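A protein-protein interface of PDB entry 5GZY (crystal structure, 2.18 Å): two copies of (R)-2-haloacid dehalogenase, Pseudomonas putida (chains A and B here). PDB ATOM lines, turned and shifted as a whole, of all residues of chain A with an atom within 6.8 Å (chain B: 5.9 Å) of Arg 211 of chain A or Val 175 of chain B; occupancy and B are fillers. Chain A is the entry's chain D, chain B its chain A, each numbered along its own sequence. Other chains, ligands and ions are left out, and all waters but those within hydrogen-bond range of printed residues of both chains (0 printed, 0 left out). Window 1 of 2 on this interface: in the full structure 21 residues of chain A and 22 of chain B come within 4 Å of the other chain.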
ATOM      1  N   TYR A 112      15.619 -22.651  16.471  1.00  0.00           N
ATOM      2  CA  TYR A 112      16.111 -21.722  15.452  1.00  0.00           C
ATOM      3  C   TYR A 112      15.873 -22.234  14.038  1.00  0.00           C
ATOM      4  O   TYR A 112      16.235 -23.358  13.707  1.00  0.00           O
ATOM      5  CB  TYR A 112      17.605 -21.449  15.648  1.00  0.00           C
ATOM      6  CG  TYR A 112      17.909 -20.537  16.813  1.00  0.00           C
ATOM      7  CD1 TYR A 112      18.079 -21.047  18.090  1.00  0.00           C
ATOM      8  CD2 TYR A 112      18.018 -19.161  16.634  1.00  0.00           C
ATOM      9  CE1 TYR A 112      18.354 -20.211  19.162  1.00  0.00           C
ATOM     10  CE2 TYR A 112      18.295 -18.328  17.686  1.00  0.00           C
ATOM     11  CZ  TYR A 112      18.458 -18.850  18.954  1.00  0.00           C
ATOM     12  OH  TYR A 112      18.731 -18.014  20.012  1.00  0.00           O
ATOM     13  N   GLU A 116      17.070 -17.964  10.467  1.00  0.00           N
ATOM     14  CA  GLU A 116      17.624 -17.344  11.653  1.00  0.00           C
ATOM     15  C   GLU A 116      19.110 -17.679  11.795  1.00  0.00           C
ATOM     16  O   GLU A 116      19.919 -16.807  12.087  1.00  0.00           O
ATOM     17  CB  GLU A 116      16.856 -17.777  12.893  1.00  0.00           C
ATOM     18  CG  GLU A 116      15.516 -17.071  13.058  1.00  0.00           C
ATOM     19  CD  GLU A 116      14.736 -17.601  14.230  1.00  0.00           C
ATOM     20  OE1 GLU A 116      14.890 -18.793  14.559  1.00  0.00           O
ATOM     21  OE2 GLU A 116      13.977 -16.823  14.831  1.00  0.00           O
ATOM     22  N   GLN A 119      21.049 -15.655   9.537  1.00  0.00           N
ATOM     23  CA  GLN A 119      21.227 -14.293  10.039  1.00  0.00           C
ATOM     24  C   GLN A 119      22.351 -14.220  11.072  1.00  0.00           C
ATOM     25  O   GLN A 119      23.091 -13.244  11.132  1.00  0.00           O
ATOM     26  CB  GLN A 119      19.927 -13.762  10.652  1.00  0.00           C
ATOM     27  CG  GLN A 119      18.800 -13.549   9.657  1.00  0.00           C
ATOM     28  CD  GLN A 119      17.501 -13.151  10.341  1.00  0.00           C
ATOM     29  OE1 GLN A 119      17.433 -13.068  11.563  1.00  0.00           O
ATOM     30  NE2 GLN A 119      16.465 -12.916   9.555  1.00  0.00           N
ATOM     31  N   VAL A 123      26.002 -11.999  10.825  1.00  0.00           N
ATOM     32  CA  VAL A 123      26.525 -11.164  11.892  1.00  0.00           C
ATOM     33  C   VAL A 123      27.974 -11.557  12.224  1.00  0.00           C
ATOM     34  O   VAL A 123      28.847 -10.704  12.314  1.00  0.00           O
ATOM     35  CB  VAL A 123      25.637 -11.259  13.155  1.00  0.00           C
ATOM     36  CG1 VAL A 123      26.319 -10.642  14.338  1.00  0.00           C
ATOM     37  CG2 VAL A 123      24.298 -10.576  12.913  1.00  0.00           C
ATOM     38  N   VAL A 175      22.561  -4.702  15.274  1.00  0.00           N
ATOM     39  CA  VAL A 175      21.825  -4.659  16.522  1.00  0.00           C
ATOM     40  C   VAL A 175      22.691  -5.191  17.651  1.00  0.00           C
ATOM     41  O   VAL A 175      23.112  -6.345  17.634  1.00  0.00           O
ATOM     42  CB  VAL A 175      20.531  -5.491  16.461  1.00  0.00           C
ATOM     43  CG1 VAL A 175      19.837  -5.477  17.800  1.00  0.00           C
ATOM     44  CG2 VAL A 175      19.607  -4.988  15.347  1.00  0.00           C
ATOM     45  N   MET A 176      22.951  -4.341  18.630  1.00  0.00           N
ATOM     46  CA  MET A 176      23.797  -4.693  19.759  1.00  0.00           C
ATOM     47  C   MET A 176      23.069  -4.446  21.063  1.00  0.00           C
ATOM     48  O   MET A 176      22.473  -3.391  21.251  1.00  0.00           O
ATOM     49  CB  MET A 176      25.092  -3.889  19.726  1.00  0.00           C
ATOM     50  CG  MET A 176      26.019  -4.269  18.587  1.00  0.00           C
ATOM     51  SD  MET A 176      27.482  -3.229  18.515  1.00  0.00           S
ATOM     52  CE  MET A 176      26.769  -1.662  18.031  1.00  0.00           C
ATOM     53  N   VAL A 177      23.114  -5.423  21.960  1.00  0.00           N
ATOM     54  CA  VAL A 177      22.457  -5.282  23.237  1.00  0.00           C
ATOM     55  C   VAL A 177      23.432  -4.675  24.235  1.00  0.00           C
ATOM     56  O   VAL A 177      24.271  -5.372  24.814  1.00  0.00           O
ATOM     57  CB  VAL A 177      21.917  -6.610  23.762  1.00  0.00           C
ATOM     58  CG1 VAL A 177      21.096  -6.360  24.990  1.00  0.00           C
ATOM     59  CG2 VAL A 177      21.062  -7.302  22.694  1.00  0.00           C
ATOM     60  N   LEU A 186      21.576 -11.744  31.134  1.00  0.00           N
ATOM     61  CA  LEU A 186      22.486 -11.297  30.106  1.00  0.00           C
ATOM     62  C   LEU A 186      23.667 -10.608  30.778  1.00  0.00           C
ATOM     63  O   LEU A 186      24.814 -10.840  30.412  1.00  0.00           O
ATOM     64  CB  LEU A 186      21.791 -10.378  29.123  1.00  0.00           C
ATOM     65  CG  LEU A 186      22.574 -10.092  27.850  1.00  0.00           C
ATOM     66  CD1 LEU A 186      22.979 -11.385  27.179  1.00  0.00           C
ATOM     67  CD2 LEU A 186      21.716  -9.278  26.918  1.00  0.00           C
ATOM     68  N   TYR A 190      27.467 -11.460  30.413  1.00  0.00           N
ATOM     69  CA  TYR A 190      28.404 -10.380  30.200  1.00  0.00           C
ATOM     70  C   TYR A 190      29.472 -10.376  31.294  1.00  0.00           C
ATOM     71  O   TYR A 190      30.643 -10.147  31.010  1.00  0.00           O
ATOM     72  CB  TYR A 190      27.679  -9.042  30.147  1.00  0.00           C
ATOM     73  CG  TYR A 190      26.984  -8.755  28.832  1.00  0.00           C
ATOM     74  CD1 TYR A 190      27.106  -9.614  27.745  1.00  0.00           C
ATOM     75  CD2 TYR A 190      26.211  -7.616  28.675  1.00  0.00           C
ATOM     76  CE1 TYR A 190      26.479  -9.341  26.543  1.00  0.00           C
ATOM     77  CE2 TYR A 190      25.584  -7.334  27.481  1.00  0.00           C
ATOM     78  CZ  TYR A 190      25.716  -8.194  26.420  1.00  0.00           C
ATOM     79  OH  TYR A 190      25.079  -7.901  25.239  1.00  0.00           O
ATOM     80  N   TYR A 206      29.993  -9.567  20.943  1.00  0.00           N
ATOM     81  CA  TYR A 206      29.139 -10.313  21.862  1.00  0.00           C
ATOM     82  C   TYR A 206      27.789  -9.604  22.102  1.00  0.00           C
ATOM     83  O   TYR A 206      26.780 -10.259  22.351  1.00  0.00           O
ATOM     84  CB  TYR A 206      29.854 -10.569  23.195  1.00  0.00           C
ATOM     85  CG  TYR A 206      31.307 -10.989  23.053  1.00  0.00           C
ATOM     86  CD1 TYR A 206      31.656 -12.123  22.327  1.00  0.00           C
ATOM     87  CD2 TYR A 206      32.332 -10.249  23.643  1.00  0.00           C
ATOM     88  CE1 TYR A 206      32.985 -12.505  22.180  1.00  0.00           C
ATOM     89  CE2 TYR A 206      33.660 -10.628  23.513  1.00  0.00           C
ATOM     90  CZ  TYR A 206      33.981 -11.758  22.775  1.00  0.00           C
ATOM     91  OH  TYR A 206      35.291 -12.140  22.619  1.00  0.00           O
ATOM     92  N   LYS A 207      27.776  -8.276  22.006  1.00  0.00           N
ATOM     93  CA  LYS A 207      26.539  -7.515  22.136  1.00  0.00           C
ATOM     94  C   LYS A 207      25.629  -7.800  20.949  1.00  0.00           C
ATOM     95  O   LYS A 207      24.416  -7.811  21.099  1.00  0.00           O
ATOM     96  CB  LYS A 207      26.808  -5.999  22.252  1.00  0.00           C
ATOM     97  CG  LYS A 207      27.486  -5.568  23.552  1.00  0.00           C
ATOM     98  CD  LYS A 207      27.654  -4.039  23.665  1.00  0.00           C
ATOM     99  CE  LYS A 207      28.577  -3.485  22.586  1.00  0.00           C
ATOM    100  NZ  LYS A 207      28.874  -2.028  22.687  1.00  0.00           N
ATOM    101  N   ALA A 208      26.217  -8.040  19.780  1.00  0.00           N
ATOM    102  CA  ALA A 208      25.438  -8.355  18.580  1.00  0.00           C
ATOM    103  C   ALA A 208      24.920  -9.786  18.621  1.00  0.00           C
ATOM    104  O   ALA A 208      23.795 -10.054  18.204  1.00  0.00           O
ATOM    105  CB  ALA A 208      26.265  -8.132  17.300  1.00  0.00           C
ATOM    106  N   MET A 209      25.748 -10.708  19.104  1.00  0.00           N
ATOM    107  CA  MET A 209      25.298 -12.078  19.290  1.00  0.00           C
ATOM    108  C   MET A 209      24.175 -12.107  20.310  1.00  0.00           C
ATOM    109  O   MET A 209      23.278 -12.933  20.223  1.00  0.00           O
ATOM    110  CB  MET A 209      26.446 -12.979  19.741  1.00  0.00           C
ATOM    111  CG  MET A 209      27.521 -13.101  18.707  1.00  0.00           C
ATOM    112  SD  MET A 209      29.046 -13.747  19.368  1.00  0.00           S
ATOM    113  CE  MET A 209      30.183 -12.904  18.285  1.00  0.00           C
ATOM    114  N   ALA A 210      24.231 -11.179  21.261  1.00  0.00           N
ATOM    115  CA  ALA A 210      23.254 -11.122  22.337  1.00  0.00           C
ATOM    116  C   ALA A 210      21.852 -10.753  21.852  1.00  0.00           C
ATOM    117  O   ALA A 210      20.891 -10.892  22.607  1.00  0.00           O
ATOM    118  CB  ALA A 210      23.717 -10.143  23.425  1.00  0.00           C
ATOM    119  N   ARG A 211      21.729 -10.297  20.603  1.00  0.00           N
ATOM    120  CA  ARG A 211      20.415 -10.187  19.960  1.00  0.00           C
ATOM    121  C   ARG A 211      19.647 -11.518  20.072  1.00  0.00           C
ATOM    122  O   ARG A 211      18.417 -11.543  20.099  1.00  0.00           O
ATOM    123  CB  ARG A 211      20.561  -9.769  18.494  1.00  0.00           C
ATOM    124  CG  ARG A 211      19.639 -10.491  17.487  1.00  0.00           C
ATOM    125  CD  ARG A 211      18.432  -9.696  17.305  1.00  0.00           C
ATOM    126  NE  ARG A 211      17.389 -10.228  16.425  1.00  0.00           N
ATOM    127  CZ  ARG A 211      16.359 -10.962  16.833  1.00  0.00           C
ATOM    128  NH1 ARG A 211      16.273 -11.338  18.101  1.00  0.00           N
ATOM    129  NH2 ARG A 211      15.419 -11.317  15.970  1.00  0.00           N
ATOM    130  N   TRP A 212      20.389 -12.619  20.133  1.00  0.00           N
ATOM    131  CA  TRP A 212      19.821 -13.949  20.345  1.00  0.00           C
ATOM    132  C   TRP A 212      20.457 -14.540  21.599  1.00  0.00           C
ATOM    133  O   TRP A 212      21.388 -15.335  21.500  1.00  0.00           O
ATOM    134  CB  TRP A 212      20.083 -14.869  19.157  1.00  0.00           C
ATOM    135  CG  TRP A 212      19.648 -14.370  17.817  1.00  0.00           C
ATOM    136  CD1 TRP A 212      18.411 -14.503  17.262  1.00  0.00           C
ATOM    137  CD2 TRP A 212      20.460 -13.719  16.830  1.00  0.00           C
ATOM    138  NE1 TRP A 212      18.394 -13.951  16.005  1.00  0.00           N
ATOM    139  CE2 TRP A 212      19.643 -13.470  15.711  1.00  0.00           C
ATOM    140  CE3 TRP A 212      21.799 -13.299  16.794  1.00  0.00           C
ATOM    141  CZ2 TRP A 212      20.109 -12.819  14.571  1.00  0.00           C
ATOM    142  CZ3 TRP A 212      22.263 -12.664  15.652  1.00  0.00           C
ATOM    143  CH2 TRP A 212      21.420 -12.439  14.554  1.00  0.00           C
ATOM    144  N   PRO A 213      19.971 -14.129  22.780  1.00  0.00           N
ATOM    145  CA  PRO A 213      20.594 -14.490  24.050  1.00  0.00           C
ATOM    146  C   PRO A 213      20.877 -15.983  24.190  1.00  0.00           C
ATOM    147  O   PRO A 213      21.934 -16.330  24.689  1.00  0.00           O
ATOM    148  CB  PRO A 213      19.563 -14.031  25.076  1.00  0.00           C
ATOM    149  CG  PRO A 213      18.908 -12.862  24.423  1.00  0.00           C
ATOM    150  CD  PRO A 213      18.783 -13.284  22.978  1.00  0.00           C
ATOM    151  N   SER A 214      19.971 -16.846  23.742  1.00  0.00           N
ATOM    152  CA  SER A 214      20.183 -18.283  23.911  1.00  0.00           C
ATOM    153  C   SER A 214      21.292 -18.777  22.985  1.00  0.00           C
ATOM    154  O   SER A 214      22.004 -19.713  23.320  1.00  0.00           O
ATOM    155  CB  SER A 214      18.894 -19.072  23.669  1.00  0.00           C
ATOM    156  OG  SER A 214      18.492 -19.000  22.320  1.00  0.00           O
ATOM    157  N   LEU A 216      23.994 -16.786  22.083  1.00  0.00           N
ATOM    158  CA  LEU A 216      25.225 -16.315  22.711  1.00  0.00           C
ATOM    159  C   LEU A 216      25.637 -17.270  23.826  1.00  0.00           C
ATOM    160  O   LEU A 216      26.799 -17.657  23.915  1.00  0.00           O
ATOM    161  CB  LEU A 216      25.074 -14.891  23.263  1.00  0.00           C
ATOM    162  CG  LEU A 216      26.242 -14.402  24.140  1.00  0.00           C
ATOM    163  CD1 LEU A 216      27.551 -14.429  23.386  1.00  0.00           C
ATOM    164  CD2 LEU A 216      25.993 -13.000  24.690  1.00  0.00           C
ATOM    165  N   ILE B 173      11.342  -6.117   8.778  1.00  0.00           N
ATOM    166  CA  ILE B 173      10.656  -6.745   9.894  1.00  0.00           C
ATOM    167  C   ILE B 173      11.307  -6.220  11.174  1.00  0.00           C
ATOM    168  O   ILE B 173      12.526  -6.186  11.273  1.00  0.00           O
ATOM    169  CB  ILE B 173      10.730  -8.284   9.826  1.00  0.00           C
ATOM    170  CG1 ILE B 173      10.124  -8.784   8.514  1.00  0.00           C
ATOM    171  CG2 ILE B 173      10.004  -8.923  11.009  1.00  0.00           C
ATOM    172  CD1 ILE B 173      10.246 -10.293   8.295  1.00  0.00           C
ATOM    173  N   PRO B 174      10.498  -5.757  12.138  1.00  0.00           N
ATOM    174  CA  PRO B 174      11.126  -5.259  13.364  1.00  0.00           C
ATOM    175  C   PRO B 174      11.884  -6.354  14.087  1.00  0.00           C
ATOM    176  O   PRO B 174      11.536  -7.520  13.963  1.00  0.00           O
ATOM    177  CB  PRO B 174       9.943  -4.751  14.200  1.00  0.00           C
ATOM    178  CG  PRO B 174       8.712  -5.130  13.460  1.00  0.00           C
ATOM    179  CD  PRO B 174       9.071  -5.415  12.055  1.00  0.00           C
ATOM    180  N   VAL B 175      12.935  -5.975  14.797  1.00  0.00           N
ATOM    181  CA  VAL B 175      13.717  -6.922  15.581  1.00  0.00           C
ATOM    182  C   VAL B 175      12.886  -7.413  16.751  1.00  0.00           C
ATOM    183  O   VAL B 175      12.413  -6.626  17.565  1.00  0.00           O
ATOM    184  CB  VAL B 175      15.022  -6.302  16.100  1.00  0.00           C
ATOM    185  CG1 VAL B 175      15.750  -7.285  17.027  1.00  0.00           C
ATOM    186  CG2 VAL B 175      15.921  -5.880  14.928  1.00  0.00           C
ATOM    187  N   MET B 176      12.698  -8.721  16.812  1.00  0.00           N
ATOM    188  CA  MET B 176      11.857  -9.337  17.825  1.00  0.00           C
ATOM    189  C   MET B 176      12.589 -10.462  18.532  1.00  0.00           C
ATOM    190  O   MET B 176      13.158 -11.342  17.889  1.00  0.00           O
ATOM    191  CB  MET B 176      10.566  -9.859  17.200  1.00  0.00           C
ATOM    192  CG  MET B 176       9.566  -8.766  16.830  1.00  0.00           C
ATOM    193  SD  MET B 176       8.104  -9.393  15.965  1.00  0.00           S
ATOM    194  CE  MET B 176       8.842 -10.065  14.490  1.00  0.00           C
ATOM    195  N   VAL B 177      12.585 -10.428  19.859  1.00  0.00           N
ATOM    196  CA  VAL B 177      13.267 -11.465  20.611  1.00  0.00           C
ATOM    197  C   VAL B 177      12.268 -12.585  20.867  1.00  0.00           C
ATOM    198  O   VAL B 177      11.463 -12.532  21.796  1.00  0.00           O
ATOM    199  CB  VAL B 177      13.865 -10.951  21.938  1.00  0.00           C
ATOM    200  CG1 VAL B 177      14.677 -12.058  22.602  1.00  0.00           C
ATOM    201  CG2 VAL B 177      14.744  -9.713  21.710  1.00  0.00           C
ATOM    202  N   GLU B 178      12.317 -13.582  19.990  1.00  0.00           N
ATOM    203  CA  GLU B 178      11.450 -14.741  20.053  1.00  0.00           C
ATOM    204  C   GLU B 178      11.680 -15.525  21.344  1.00  0.00           C
ATOM    205  O   GLU B 178      12.740 -15.422  21.957  1.00  0.00           O
ATOM    206  CB  GLU B 178      11.685 -15.629  18.835  1.00  0.00           C
ATOM    207  CG  GLU B 178      11.478 -14.935  17.493  1.00  0.00           C
ATOM    208  CD  GLU B 178      10.041 -14.482  17.250  1.00  0.00           C
ATOM    209  OE1 GLU B 178       9.110 -15.053  17.847  1.00  0.00           O
ATOM    210  OE2 GLU B 178       9.851 -13.546  16.459  1.00  0.00           O
ATOM    211  N   HIS B 181      14.734 -17.393  21.448  1.00  0.00           N
ATOM    212  CA  HIS B 181      15.906 -16.515  21.558  1.00  0.00           C
ATOM    213  C   HIS B 181      16.141 -16.171  23.021  1.00  0.00           C
ATOM    214  O   HIS B 181      17.267 -16.030  23.457  1.00  0.00           O
ATOM    215  CB  HIS B 181      15.737 -15.197  20.783  1.00  0.00           C
ATOM    216  CG  HIS B 181      15.383 -15.368  19.339  1.00  0.00           C
ATOM    217  ND1 HIS B 181      14.992 -14.308  18.544  1.00  0.00           N
ATOM    218  CD2 HIS B 181      15.358 -16.463  18.546  1.00  0.00           C
ATOM    219  CE1 HIS B 181      14.746 -14.747  17.325  1.00  0.00           C
ATOM    220  NE2 HIS B 181      14.959 -16.052  17.299  1.00  0.00           N
ATOM    221  N   LYS B 207       7.800  -8.527  22.146  1.00  0.00           N
ATOM    222  CA  LYS B 207       9.046  -9.103  21.643  1.00  0.00           C
ATOM    223  C   LYS B 207       9.949  -8.046  21.011  1.00  0.00           C
ATOM    224  O   LYS B 207      11.168  -8.165  21.076  1.00  0.00           O
ATOM    225  CB  LYS B 207       8.777 -10.227  20.619  1.00  0.00           C
ATOM    226  CG  LYS B 207       8.171 -11.510  21.206  1.00  0.00           C
ATOM    227  CD  LYS B 207       8.019 -12.645  20.153  1.00  0.00           C
ATOM    228  CE  LYS B 207       7.026 -12.289  19.041  1.00  0.00           C
ATOM    229  NZ  LYS B 207       6.775 -13.394  18.067  1.00  0.00           N
ATOM    230  N   ALA B 208       9.354  -7.028  20.392  1.00  0.00           N
ATOM    231  CA  ALA B 208      10.138  -5.960  19.774  1.00  0.00           C
ATOM    232  C   ALA B 208      10.661  -4.995  20.842  1.00  0.00           C
ATOM    233  O   ALA B 208      11.777  -4.512  20.754  1.00  0.00           O
ATOM    234  CB  ALA B 208       9.311  -5.208  18.729  1.00  0.00           C
ATOM    235  N   MET B 209       9.851  -4.719  21.853  1.00  0.00           N
ATOM    236  CA  MET B 209      10.327  -3.921  22.978  1.00  0.00           C
ATOM    237  C   MET B 209      11.467  -4.635  23.696  1.00  0.00           C
ATOM    238  O   MET B 209      12.364  -3.999  24.238  1.00  0.00           O
ATOM    239  CB  MET B 209       9.188  -3.630  23.950  1.00  0.00           C
ATOM    240  CG  MET B 209       8.074  -2.807  23.329  1.00  0.00           C
ATOM    241  SD  MET B 209       6.549  -2.877  24.290  1.00  0.00           S
ATOM    242  CE  MET B 209       5.364  -2.795  22.959  1.00  0.00           C
ATOM    243  N   ARG B 211      13.937  -6.109  22.543  1.00  0.00           N
ATOM    244  CA  ARG B 211      15.247  -5.743  21.986  1.00  0.00           C
ATOM    245  C   ARG B 211      16.004  -4.877  23.010  1.00  0.00           C
ATOM    246  O   ARG B 211      17.229  -4.837  23.024  1.00  0.00           O
ATOM    247  CB  ARG B 211      15.088  -5.011  20.642  1.00  0.00           C
ATOM    248  CG  ARG B 211      15.953  -3.752  20.424  1.00  0.00           C
ATOM    249  CD  ARG B 211      17.193  -4.141  19.759  1.00  0.00           C
ATOM    250  NE  ARG B 211      18.216  -3.105  19.546  1.00  0.00           N
ATOM    251  CZ  ARG B 211      19.204  -2.842  20.396  1.00  0.00           C
ATOM    252  NH1 ARG B 211      19.256  -3.460  21.567  1.00  0.00           N
ATOM    253  NH2 ARG B 211      20.125  -1.946  20.084  1.00  0.00           N
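N of Pro 213 of chain A sits close to O of His 181 of chain B, 3.4 Å away.
A ring nitrogen (ND1) of His 181 of chain B sits at hydrogen-bond distance from the guanidinium group (NH1) of Arg 211 of chain A (3.3 Å).
NH2 of Arg 211 of chain B lies within hydrogen-bond range of O of Met 176 of chain A (3.0 Å).
The backbone carbonyl oxygen (O) of Met 176 of chain B sits at hydrogen-bond distance from the guanidinium group (NH2) of Arg 211 of chain A (3.0 Å).
The side-chain carboxylate of Glu 116 of chain A sits at hydrogen-bond distance from a ring nitrogen (NE2) of His 181 of chain B (2.8 Å).
The backbone carbonyl oxygen (O) of His 181 of chain B is in hydrogen-bond range of the backbone NH (N) of Ser 214 of chain A.
Val 175 of chain B touches its own counterpart, Val 175 of chain A.
Val 175 of chain A touches Arg 211 of chain B, and with the chains exchanged Arg 211 of chain A touches Val 175 of chain B.
Met 176 of chain A touches Arg 211 of chain B, and with the chains exchanged Arg 211 of chain A touches Met 176 of chain B.
Arg 211 of chain A touches Val 177 of chain B, but with the chains exchanged Val 177 of chain A does not touch Arg 211 of chain B (4.04 Å).
Of the 12 pairs that touch across the chains among the printed residues, 5 have their exchanged pair printed and touching as well.
Of chain B, only Val 175 (3.4 Å), Met 176 (3.0 Å), Val 177 (3.9 Å) and His 181 (3.3 Å) come within 4 Å of Arg 211 of chain A.
Of chain A, only Val 175 and Arg 211 come within 4 Å of Val 175 of chain B.
Of the printed residues of chain A, Arg 211 of chain B touches Val 175 and Met 176.
Of the printed residues of chain B, Ser 214 of chain A touches His 181 (2.8 Å).
Printed residues of chain A within 4 Å of Met 176 of chain B: Arg 211 (3.0 Å).
Met 209 of chain B touches none of the printed residues of chain A.
Hydrophobic or aromatic side chains of chain A within 4 Å of the printed part of chain B: Tyr 112, Val 175, Trp 212 and Pro 213.
Of the 11 printed residues of chain B, 5 touch a printed residue of chain A.
Hydrophobic or aromatic side chains of chain B that line the printed part of chain A: Val 175 and His 181.
The backbone carbonyl oxygen of Lys 207 of chain B lies within hydrogen-bond range of the backbone NH of Val 177 of chain B.
OH of Tyr 112 of chain A lies within hydrogen-bond range of OG of Ser 214 of chain A, 2.5 Å away.
N of Glu 178 of chain B is in hydrogen-bond range of ND1 of His 181 of chain B, at 3.1 Å.
OH of Tyr 112 of chain A touches CA of His 181 of chain B, at 3.6 Å.
CG2 of Val 175 of chain A touches CG2 of Val 175 of chain B, at 3.8 Å.
CG1 of Val 175 of chain A touches NE of Arg 211 of chain B (3.4 Å).
Arg 211 of chain A touches Val 175 of chain B.
Arg 211 of chain A touches Val 177 of chain B (NH1 to CA, 3.9 Å).
Trp 212 of chain A touches His 181 of chain B.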
